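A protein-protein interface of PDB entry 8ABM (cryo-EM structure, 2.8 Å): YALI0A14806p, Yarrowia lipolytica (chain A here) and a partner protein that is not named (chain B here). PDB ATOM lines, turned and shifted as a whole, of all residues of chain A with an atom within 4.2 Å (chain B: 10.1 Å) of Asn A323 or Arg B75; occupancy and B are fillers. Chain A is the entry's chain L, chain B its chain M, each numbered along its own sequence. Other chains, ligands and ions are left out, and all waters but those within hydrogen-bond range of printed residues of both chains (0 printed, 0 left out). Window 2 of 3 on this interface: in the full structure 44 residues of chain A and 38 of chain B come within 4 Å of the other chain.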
ATOM      1  N   HIS A 316      -5.883 -28.704   8.164  1.00  0.00           N
ATOM      2  CA  HIS A 316      -6.315 -28.860   9.538  1.00  0.00           C
ATOM      3  C   HIS A 316      -7.432 -27.893   9.902  1.00  0.00           C
ATOM      4  O   HIS A 316      -7.855 -27.861  11.055  1.00  0.00           O
ATOM      5  CB  HIS A 316      -5.114 -28.667  10.451  1.00  0.00           C
ATOM      6  CG  HIS A 316      -4.140 -29.772  10.293  1.00  0.00           C
ATOM      7  ND1 HIS A 316      -4.535 -31.098  10.367  1.00  0.00           N
ATOM      8  CD2 HIS A 316      -2.816 -29.766  10.035  1.00  0.00           C
ATOM      9  CE1 HIS A 316      -3.483 -31.865  10.187  1.00  0.00           C
ATOM     10  NE2 HIS A 316      -2.413 -31.074   9.980  1.00  0.00           N
ATOM     11  N   GLN A 317      -7.885 -27.097   8.934  1.00  0.00           N
ATOM     12  CA  GLN A 317      -8.875 -26.069   9.212  1.00  0.00           C
ATOM     13  C   GLN A 317     -10.196 -26.685   9.656  1.00  0.00           C
ATOM     14  O   GLN A 317     -10.534 -27.816   9.297  1.00  0.00           O
ATOM     15  CB  GLN A 317      -9.127 -25.229   7.966  1.00  0.00           C
ATOM     16  CG  GLN A 317      -7.945 -24.356   7.610  1.00  0.00           C
ATOM     17  CD  GLN A 317      -8.212 -23.515   6.388  1.00  0.00           C
ATOM     18  OE1 GLN A 317      -7.926 -22.320   6.377  1.00  0.00           O
ATOM     19  NE2 GLN A 317      -8.752 -24.127   5.342  1.00  0.00           N
ATOM     20  N   GLY A 318     -10.965 -25.895  10.405  1.00  0.00           N
ATOM     21  CA  GLY A 318     -12.180 -26.377  11.036  1.00  0.00           C
ATOM     22  C   GLY A 318     -13.384 -26.467  10.102  1.00  0.00           C
ATOM     23  O   GLY A 318     -14.291 -27.264  10.354  1.00  0.00           O
ATOM     24  N   SER A 319     -13.420 -25.584   9.096  1.00  0.00           N
ATOM     25  CA  SER A 319     -14.475 -25.486   8.095  1.00  0.00           C
ATOM     26  C   SER A 319     -14.843 -26.857   7.524  1.00  0.00           C
ATOM     27  O   SER A 319     -13.969 -27.623   7.130  1.00  0.00           O
ATOM     28  CB  SER A 319     -14.036 -24.547   7.002  1.00  0.00           C
ATOM     29  OG  SER A 319     -14.817 -24.719   5.823  1.00  0.00           O
ATOM     30  N   ARG A 320     -16.146 -27.150   7.444  1.00  0.00           N
ATOM     31  CA  ARG A 320     -16.580 -28.465   6.996  1.00  0.00           C
ATOM     32  C   ARG A 320     -16.234 -28.664   5.518  1.00  0.00           C
ATOM     33  O   ARG A 320     -15.776 -29.739   5.119  1.00  0.00           O
ATOM     34  CB  ARG A 320     -18.047 -28.696   7.374  1.00  0.00           C
ATOM     35  CG  ARG A 320     -18.657 -29.952   6.774  1.00  0.00           C
ATOM     36  CD  ARG A 320     -18.025 -31.217   7.316  1.00  0.00           C
ATOM     37  NE  ARG A 320     -18.568 -32.395   6.645  1.00  0.00           N
ATOM     38  CZ  ARG A 320     -18.129 -33.647   6.787  1.00  0.00           C
ATOM     39  NH1 ARG A 320     -17.112 -33.918   7.591  1.00  0.00           N
ATOM     40  NH2 ARG A 320     -18.709 -34.630   6.116  1.00  0.00           N
ATOM     41  N   LEU A 321     -16.400 -27.604   4.714  1.00  0.00           N
ATOM     42  CA  LEU A 321     -16.065 -27.682   3.303  1.00  0.00           C
ATOM     43  C   LEU A 321     -14.573 -27.930   3.137  1.00  0.00           C
ATOM     44  O   LEU A 321     -14.168 -28.716   2.288  1.00  0.00           O
ATOM     45  CB  LEU A 321     -16.477 -26.413   2.556  1.00  0.00           C
ATOM     46  CG  LEU A 321     -16.226 -26.468   1.044  1.00  0.00           C
ATOM     47  CD1 LEU A 321     -16.998 -27.609   0.384  1.00  0.00           C
ATOM     48  CD2 LEU A 321     -16.561 -25.149   0.377  1.00  0.00           C
ATOM     49  N   SER A 322     -13.770 -27.273   3.973  1.00  0.00           N
ATOM     50  CA  SER A 322     -12.333 -27.464   3.934  1.00  0.00           C
ATOM     51  C   SER A 322     -11.993 -28.937   4.125  1.00  0.00           C
ATOM     52  O   SER A 322     -11.175 -29.481   3.386  1.00  0.00           O
ATOM     53  CB  SER A 322     -11.656 -26.612   4.952  1.00  0.00           C
ATOM     54  OG  SER A 322     -10.252 -26.743   4.830  1.00  0.00           O
ATOM     55  N   ASN A 323     -12.643 -29.570   5.100  1.00  0.00           N
ATOM     56  CA  ASN A 323     -12.356 -30.961   5.384  1.00  0.00           C
ATOM     57  C   ASN A 323     -12.726 -31.841   4.205  1.00  0.00           C
ATOM     58  O   ASN A 323     -11.941 -32.701   3.841  1.00  0.00           O
ATOM     59  CB  ASN A 323     -12.992 -31.427   6.684  1.00  0.00           C
ATOM     60  CG  ASN A 323     -12.273 -30.796   7.851  1.00  0.00           C
ATOM     61  OD1 ASN A 323     -11.147 -31.173   8.163  1.00  0.00           O
ATOM     62  ND2 ASN A 323     -12.892 -29.814   8.481  1.00  0.00           N
ATOM     63  N   ILE A 324     -13.901 -31.618   3.614  1.00  0.00           N
ATOM     64  CA  ILE A 324     -14.369 -32.479   2.540  1.00  0.00           C
ATOM     65  C   ILE A 324     -13.419 -32.348   1.355  1.00  0.00           C
ATOM     66  O   ILE A 324     -13.085 -33.327   0.692  1.00  0.00           O
ATOM     67  CB  ILE A 324     -15.807 -32.108   2.133  1.00  0.00           C
ATOM     68  CG1 ILE A 324     -16.842 -32.455   3.206  1.00  0.00           C
ATOM     69  CG2 ILE A 324     -16.149 -32.762   0.807  1.00  0.00           C
ATOM     70  CD1 ILE A 324     -18.064 -31.557   3.200  1.00  0.00           C
ATOM     71  N   VAL A 325     -13.021 -31.111   1.083  1.00  0.00           N
ATOM     72  CA  VAL A 325     -12.255 -30.828  -0.111  1.00  0.00           C
ATOM     73  C   VAL A 325     -10.863 -31.418   0.054  1.00  0.00           C
ATOM     74  O   VAL A 325     -10.332 -31.977  -0.893  1.00  0.00           O
ATOM     75  CB  VAL A 325     -12.224 -29.318  -0.396  1.00  0.00           C
ATOM     76  CG1 VAL A 325     -11.077 -28.932  -1.315  1.00  0.00           C
ATOM     77  CG2 VAL A 325     -13.553 -28.863  -0.977  1.00  0.00           C
ATOM     78  N   SER A 326     -10.287 -31.265   1.246  1.00  0.00           N
ATOM     79  CA  SER A 326      -8.916 -31.696   1.436  1.00  0.00           C
ATOM     80  C   SER A 326      -8.820 -33.219   1.453  1.00  0.00           C
ATOM     81  O   SER A 326      -7.938 -33.765   0.793  1.00  0.00           O
ATOM     82  CB  SER A 326      -8.258 -31.040   2.615  1.00  0.00           C
ATOM     83  OG  SER A 326      -8.915 -31.400   3.813  1.00  0.00           O
ATOM     84  N   GLU A 327      -9.775 -33.890   2.119  1.00  0.00           N
ATOM     85  CA  GLU A 327      -9.761 -35.348   2.230  1.00  0.00           C
ATOM     86  C   GLU A 327      -9.935 -36.008   0.863  1.00  0.00           C
ATOM     87  O   GLU A 327      -9.371 -37.070   0.601  1.00  0.00           O
ATOM     88  CB  GLU A 327     -10.859 -35.872   3.160  1.00  0.00           C
ATOM     89  CG  GLU A 327     -10.617 -35.570   4.627  1.00  0.00           C
ATOM     90  CD  GLU A 327     -11.784 -35.902   5.547  1.00  0.00           C
ATOM     91  OE1 GLU A 327     -12.860 -35.281   5.400  1.00  0.00           O
ATOM     92  OE2 GLU A 327     -11.618 -36.796   6.401  1.00  0.00           O
ATOM     93  N   PHE B  62       5.459 -26.278  13.395  1.00  0.00           N
ATOM     94  CA  PHE B  62       4.043 -26.390  13.702  1.00  0.00           C
ATOM     95  C   PHE B  62       3.431 -27.663  13.117  1.00  0.00           C
ATOM     96  O   PHE B  62       2.242 -27.702  12.804  1.00  0.00           O
ATOM     97  CB  PHE B  62       3.313 -25.100  13.350  1.00  0.00           C
ATOM     98  CG  PHE B  62       3.844 -23.920  14.116  1.00  0.00           C
ATOM     99  CD1 PHE B  62       3.504 -23.740  15.449  1.00  0.00           C
ATOM    100  CD2 PHE B  62       4.699 -23.007  13.512  1.00  0.00           C
ATOM    101  CE1 PHE B  62       3.996 -22.657  16.168  1.00  0.00           C
ATOM    102  CE2 PHE B  62       5.213 -21.938  14.238  1.00  0.00           C
ATOM    103  CZ  PHE B  62       4.849 -21.756  15.558  1.00  0.00           C
ATOM    104  N   LYS B  68       1.121 -30.990  21.783  1.00  0.00           N
ATOM    105  CA  LYS B  68       0.024 -30.446  20.991  1.00  0.00           C
ATOM    106  C   LYS B  68       0.199 -30.858  19.536  1.00  0.00           C
ATOM    107  O   LYS B  68       1.247 -30.604  18.946  1.00  0.00           O
ATOM    108  CB  LYS B  68       0.018 -28.919  21.101  1.00  0.00           C
ATOM    109  CG  LYS B  68      -1.246 -28.196  20.653  1.00  0.00           C
ATOM    110  CD  LYS B  68      -1.078 -26.683  20.627  1.00  0.00           C
ATOM    111  CE  LYS B  68      -1.126 -25.989  21.979  1.00  0.00           C
ATOM    112  NZ  LYS B  68      -2.186 -26.507  22.880  1.00  0.00           N
ATOM    113  N   SER B  69      -0.839 -31.493  18.978  1.00  0.00           N
ATOM    114  CA  SER B  69      -0.797 -31.973  17.606  1.00  0.00           C
ATOM    115  C   SER B  69      -0.904 -30.795  16.650  1.00  0.00           C
ATOM    116  O   SER B  69      -1.413 -29.741  17.013  1.00  0.00           O
ATOM    117  CB  SER B  69      -1.894 -32.956  17.343  1.00  0.00           C
ATOM    118  OG  SER B  69      -3.149 -32.301  17.337  1.00  0.00           O
ATOM    119  N   ALA B  70      -0.451 -31.003  15.415  1.00  0.00           N
ATOM    120  CA  ALA B  70      -0.597 -29.996  14.378  1.00  0.00           C
ATOM    121  C   ALA B  70      -2.063 -29.591  14.257  1.00  0.00           C
ATOM    122  O   ALA B  70      -2.375 -28.407  14.200  1.00  0.00           O
ATOM    123  CB  ALA B  70      -0.058 -30.513  13.077  1.00  0.00           C
ATOM    124  N   LEU B  71      -2.948 -30.592  14.265  1.00  0.00           N
ATOM    125  CA  LEU B  71      -4.376 -30.348  14.181  1.00  0.00           C
ATOM    126  C   LEU B  71      -4.843 -29.470  15.337  1.00  0.00           C
ATOM    127  O   LEU B  71      -5.515 -28.474  15.109  1.00  0.00           O
ATOM    128  CB  LEU B  71      -5.116 -31.682  14.173  1.00  0.00           C
ATOM    129  CG  LEU B  71      -6.624 -31.572  14.354  1.00  0.00           C
ATOM    130  CD1 LEU B  71      -7.239 -30.820  13.189  1.00  0.00           C
ATOM    131  CD2 LEU B  71      -7.220 -32.959  14.458  1.00  0.00           C
ATOM    132  N   ARG B  72      -4.511 -29.842  16.570  1.00  0.00           N
ATOM    133  CA  ARG B  72      -5.009 -29.051  17.677  1.00  0.00           C
ATOM    134  C   ARG B  72      -4.468 -27.627  17.603  1.00  0.00           C
ATOM    135  O   ARG B  72      -5.164 -26.681  17.952  1.00  0.00           O
ATOM    136  CB  ARG B  72      -4.596 -29.626  19.023  1.00  0.00           C
ATOM    137  CG  ARG B  72      -5.266 -28.847  20.138  1.00  0.00           C
ATOM    138  CD  ARG B  72      -5.598 -29.564  21.427  1.00  0.00           C
ATOM    139  NE  ARG B  72      -6.454 -30.739  21.293  1.00  0.00           N
ATOM    140  CZ  ARG B  72      -7.647 -30.906  21.863  1.00  0.00           C
ATOM    141  NH1 ARG B  72      -8.174 -29.960  22.627  1.00  0.00           N
ATOM    142  NH2 ARG B  72      -8.310 -32.032  21.670  1.00  0.00           N
ATOM    143  N   PHE B  73      -3.220 -27.475  17.172  1.00  0.00           N
ATOM    144  CA  PHE B  73      -2.656 -26.140  17.113  1.00  0.00           C
ATOM    145  C   PHE B  73      -3.441 -25.289  16.123  1.00  0.00           C
ATOM    146  O   PHE B  73      -3.843 -24.180  16.454  1.00  0.00           O
ATOM    147  CB  PHE B  73      -1.173 -26.178  16.755  1.00  0.00           C
ATOM    148  CG  PHE B  73      -0.597 -24.805  16.530  1.00  0.00           C
ATOM    149  CD1 PHE B  73      -0.388 -23.945  17.603  1.00  0.00           C
ATOM    150  CD2 PHE B  73      -0.309 -24.354  15.247  1.00  0.00           C
ATOM    151  CE1 PHE B  73       0.104 -22.663  17.395  1.00  0.00           C
ATOM    152  CE2 PHE B  73       0.206 -23.079  15.040  1.00  0.00           C
ATOM    153  CZ  PHE B  73       0.406 -22.233  16.116  1.00  0.00           C
ATOM    154  N   VAL B  74      -3.651 -25.811  14.915  1.00  0.00           N
ATOM    155  CA  VAL B  74      -4.354 -25.053  13.897  1.00  0.00           C
ATOM    156  C   VAL B  74      -5.761 -24.678  14.363  1.00  0.00           C
ATOM    157  O   VAL B  74      -6.181 -23.547  14.150  1.00  0.00           O
ATOM    158  CB  VAL B  74      -4.371 -25.801  12.555  1.00  0.00           C
ATOM    159  CG1 VAL B  74      -5.349 -25.185  11.558  1.00  0.00           C
ATOM    160  CG2 VAL B  74      -2.980 -25.882  11.959  1.00  0.00           C
ATOM    161  N   ARG B  75      -6.501 -25.612  14.965  1.00  0.00           N
ATOM    162  CA  ARG B  75      -7.855 -25.281  15.384  1.00  0.00           C
ATOM    163  C   ARG B  75      -7.858 -24.255  16.514  1.00  0.00           C
ATOM    164  O   ARG B  75      -8.809 -23.490  16.654  1.00  0.00           O
ATOM    165  CB  ARG B  75      -8.636 -26.503  15.865  1.00  0.00           C
ATOM    166  CG  ARG B  75      -8.856 -27.562  14.804  1.00  0.00           C
ATOM    167  CD  ARG B  75      -9.803 -27.103  13.725  1.00  0.00           C
ATOM    168  NE  ARG B  75      -9.872 -28.206  12.789  1.00  0.00           N
ATOM    169  CZ  ARG B  75     -10.827 -29.123  12.780  1.00  0.00           C
ATOM    170  NH1 ARG B  75     -11.809 -29.058  13.661  1.00  0.00           N
ATOM    171  NH2 ARG B  75     -10.801 -30.093  11.884  1.00  0.00           N
ATOM    172  N   GLU B  76      -6.815 -24.223  17.338  1.00  0.00           N
ATOM    173  CA  GLU B  76      -6.847 -23.271  18.434  1.00  0.00           C
ATOM    174  C   GLU B  76      -6.381 -21.905  17.946  1.00  0.00           C
ATOM    175  O   GLU B  76      -6.794 -20.878  18.467  1.00  0.00           O
ATOM    176  CB  GLU B  76      -5.964 -23.735  19.579  1.00  0.00           C
ATOM    177  CG  GLU B  76      -6.590 -24.823  20.422  1.00  0.00           C
ATOM    178  CD  GLU B  76      -5.626 -25.376  21.463  1.00  0.00           C
ATOM    179  OE1 GLU B  76      -6.086 -26.054  22.410  1.00  0.00           O
ATOM    180  OE2 GLU B  76      -4.407 -25.114  21.339  1.00  0.00           O
ATOM    181  N   LEU B  77      -5.487 -21.899  16.963  1.00  0.00           N
ATOM    182  CA  LEU B  77      -5.001 -20.651  16.414  1.00  0.00           C
ATOM    183  C   LEU B  77      -6.136 -19.950  15.663  1.00  0.00           C
ATOM    184  O   LEU B  77      -6.162 -18.726  15.614  1.00  0.00           O
ATOM    185  CB  LEU B  77      -3.805 -21.002  15.525  1.00  0.00           C
ATOM    186  CG  LEU B  77      -3.371 -19.985  14.475  1.00  0.00           C
ATOM    187  CD1 LEU B  77      -2.179 -19.194  14.977  1.00  0.00           C
ATOM    188  CD2 LEU B  77      -2.999 -20.692  13.179  1.00  0.00           C
ATOM    189  N   GLU B  78      -7.095 -20.723  15.125  1.00  0.00           N
ATOM    190  CA  GLU B  78      -8.286 -20.176  14.483  1.00  0.00           C
ATOM    191  C   GLU B  78      -9.228 -19.554  15.511  1.00  0.00           C
ATOM    192  O   GLU B  78      -9.960 -18.631  15.182  1.00  0.00           O
ATOM    193  CB  GLU B  78      -9.075 -21.247  13.724  1.00  0.00           C
ATOM    194  CG  GLU B  78      -8.445 -21.696  12.415  1.00  0.00           C
ATOM    195  CD  GLU B  78      -9.145 -22.863  11.714  1.00  0.00           C
ATOM    196  OE1 GLU B  78      -9.622 -22.690  10.559  1.00  0.00           O
ATOM    197  OE2 GLU B  78      -9.171 -23.966  12.320  1.00  0.00           O
ATOM    198  N   LEU B  79      -9.221 -20.043  16.753  1.00  0.00           N
ATOM    199  CA  LEU B  79     -10.032 -19.435  17.796  1.00  0.00           C
ATOM    200  C   LEU B  79      -9.443 -18.119  18.286  1.00  0.00           C
ATOM    201  O   LEU B  79     -10.139 -17.343  18.941  1.00  0.00           O
ATOM    202  CB  LEU B  79     -10.103 -20.394  18.976  1.00  0.00           C
ATOM    203  CG  LEU B  79     -10.849 -21.685  18.702  1.00  0.00           C
ATOM    204  CD1 LEU B  79     -10.961 -22.489  19.980  1.00  0.00           C
ATOM    205  CD2 LEU B  79     -12.233 -21.416  18.124  1.00  0.00           C
ATOM    206  N   PHE B  80      -8.147 -17.900  18.051  1.00  0.00           N
ATOM    207  CA  PHE B  80      -7.520 -16.642  18.410  1.00  0.00           C
ATOM    208  C   PHE B  80      -7.435 -15.742  17.187  1.00  0.00           C
ATOM    209  O   PHE B  80      -6.967 -14.604  17.273  1.00  0.00           O
ATOM    210  CB  PHE B  80      -6.090 -16.901  18.855  1.00  0.00           C
ATOM    211  CG  PHE B  80      -5.948 -17.311  20.291  1.00  0.00           C
ATOM    212  CD1 PHE B  80      -6.594 -16.615  21.304  1.00  0.00           C
ATOM    213  CD2 PHE B  80      -5.148 -18.386  20.631  1.00  0.00           C
ATOM    214  CE1 PHE B  80      -6.415 -16.964  22.634  1.00  0.00           C
ATOM    215  CE2 PHE B  80      -4.991 -18.759  21.955  1.00  0.00           C
ATOM    216  CZ  PHE B  80      -5.625 -18.051  22.956  1.00  0.00           C
ATOM    217  N   GLY B  81      -7.852 -16.311  16.050  1.00  0.00           N
ATOM    218  CA  GLY B  81      -7.766 -15.684  14.744  1.00  0.00           C
ATOM    219  C   GLY B  81      -6.344 -15.271  14.365  1.00  0.00           C
ATOM    220  O   GLY B  81      -6.174 -14.402  13.514  1.00  0.00           O
ATOM    221  N   GLY B  82      -5.337 -15.886  14.999  1.00  0.00           N
ATOM    222  CA  GLY B  82      -3.944 -15.724  14.602  1.00  0.00           C
ATOM    223  C   GLY B  82      -3.637 -16.267  13.205  1.00  0.00           C
ATOM    224  O   GLY B  82      -4.387 -17.055  12.635  1.00  0.00           O
ATOM    225  N   LEU B  84      -0.129 -17.664  10.723  1.00  0.00           N
ATOM    226  CA  LEU B  84       1.210 -18.200  10.826  1.00  0.00           C
ATOM    227  C   LEU B  84       1.929 -18.046   9.492  1.00  0.00           C
ATOM    228  O   LEU B  84       1.366 -18.329   8.445  1.00  0.00           O
ATOM    229  CB  LEU B  84       1.025 -19.655  11.227  1.00  0.00           C
ATOM    230  CG  LEU B  84       2.271 -20.515  11.219  1.00  0.00           C
ATOM    231  CD1 LEU B  84       3.236 -20.101  12.320  1.00  0.00           C
ATOM    232  CD2 LEU B  84       1.831 -21.938  11.379  1.00  0.00           C
ATOM    233  N   TYR B 106       0.116 -17.578  24.794  1.00  0.00           N
ATOM    234  CA  TYR B 106      -0.189 -18.754  24.000  1.00  0.00           C
ATOM    235  C   TYR B 106       0.894 -18.962  22.939  1.00  0.00           C
ATOM    236  O   TYR B 106       1.392 -20.075  22.764  1.00  0.00           O
ATOM    237  CB  TYR B 106      -1.595 -18.660  23.403  1.00  0.00           C
ATOM    238  CG  TYR B 106      -1.943 -19.869  22.578  1.00  0.00           C
ATOM    239  CD1 TYR B 106      -1.670 -19.886  21.219  1.00  0.00           C
ATOM    240  CD2 TYR B 106      -2.449 -21.027  23.156  1.00  0.00           C
ATOM    241  CE1 TYR B 106      -1.928 -20.998  20.437  1.00  0.00           C
ATOM    242  CE2 TYR B 106      -2.721 -22.150  22.386  1.00  0.00           C
ATOM    243  CZ  TYR B 106      -2.462 -22.132  21.023  1.00  0.00           C
ATOM    244  OH  TYR B 106      -2.721 -23.218  20.238  1.00  0.00           O
ATOM    245  N   PHE B 107       1.227 -17.891  22.216  1.00  0.00           N
ATOM    246  CA  PHE B 107       2.134 -17.987  21.088  1.00  0.00           C
ATOM    247  C   PHE B 107       3.567 -18.211  21.537  1.00  0.00           C
ATOM    248  O   PHE B 107       4.319 -18.862  20.819  1.00  0.00           O
ATOM    249  CB  PHE B 107       1.960 -16.804  20.137  1.00  0.00           C
ATOM    250  CG  PHE B 107       0.622 -16.904  19.476  1.00  0.00           C
ATOM    251  CD1 PHE B 107       0.450 -17.747  18.389  1.00  0.00           C
ATOM    252  CD2 PHE B 107      -0.488 -16.282  20.033  1.00  0.00           C
ATOM    253  CE1 PHE B 107      -0.804 -17.899  17.817  1.00  0.00           C
ATOM    254  CE2 PHE B 107      -1.744 -16.450  19.470  1.00  0.00           C
ATOM    255  CZ  PHE B 107      -1.897 -17.248  18.352  1.00  0.00           C
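Printed residues of chain B within 4 Å of His A316: Ala B70 (3.9 Å), Leu B71 (3.7 Å), Val B74 (3.6 Å) and Arg B75 (2.7 Å).
Of chain B, only Arg B75 (3.4 Å) and Glu B78 (3.3 Å) come within 4 Å of Gly A318.
No residue of chain B comes within 4 Å of Ser A319.
Ser A322 touches none of the printed residues of chain B.
Asn A323 touches one residue of chain B.
No residue of chain B comes within 4 Å of Ile A324.
No residue of chain B comes within 4 Å of Ser A326.
Glu A327 touches none of the printed residues of chain B.
Lys B68 touches none of the printed residues of chain A.
Of the printed residues of chain A, Leu B71 touches His A316 (3.7 Å).
Arg B75 touches just these residues of chain A: His A316 (2.7 Å), Gln A317 (3.5 Å), Gly A318 (3.4 Å) and Asn A323 (3.9 Å).
Leu B84 touches none of the printed residues of chain A.
The nearest residue of chain B that does not touch Asn A323 is Leu B71 (6.4 Å).
The nearest printed residue of chain A that does not touch Ala B70 is Gln A317 (7.7 Å).
The side-chain amide nitrogen of Gln A317 is in hydrogen-bond range of the side-chain hydroxyl of Ser A322 (3.1 Å).
ND2 of Asn A323 sits at hydrogen-bond distance from O of Gln A317 (3.2 Å).
The backbone carbonyl oxygen (O) of Gly A318 sits at hydrogen-bond distance from the side-chain amide nitrogen (ND2) of Asn A323, 3.5 Å away.
O of Ser A319 lies within hydrogen-bond range of ND2 of Asn A323 (2.8 Å).
O of Asn A323 is in hydrogen-bond range of OG of Ser A326, at 3.3 Å.
The backbone carbonyl oxygen (O) of His A316 is in hydrogen-bond range of the guanidinium group (NE) of Arg B75 (2.7 Å).
The backbone carbonyl oxygen (O) of Gln A317 lies within hydrogen-bond range of the guanidinium group (NH2) of Arg B75.
The backbone NH (N) of Gly A318 lies within hydrogen-bond range of the side-chain carboxylate (OE2) of Glu B78.
NE of Arg B75 sits close to N of Gly A318.
CB of Ala B70 touches NE2 of His A316, 3.9 Å away.
His A316 touches Leu B71 (O to CD1, 3.7 Å).
His A316 touches Val B74 (CB to CB, 3.6 Å).
CB of Gln A317 touches OE1 of Glu B78, 3.7 Å away.
OD1 of Asn A323 touches NH2 of Arg B75, 3.9 Å away.
Of the 12 printed residues of chain A, 4 touch a printed residue of chain B.
Of the 19 printed residues of chain B, 5 touch a printed residue of chain A.
Hydrophobic or aromatic side chains of chain B within 4 Å of the printed part of chain A: Ala B70, Leu B71 and Val B74.
Among the printed residues, 9 pairs touch across the chains.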
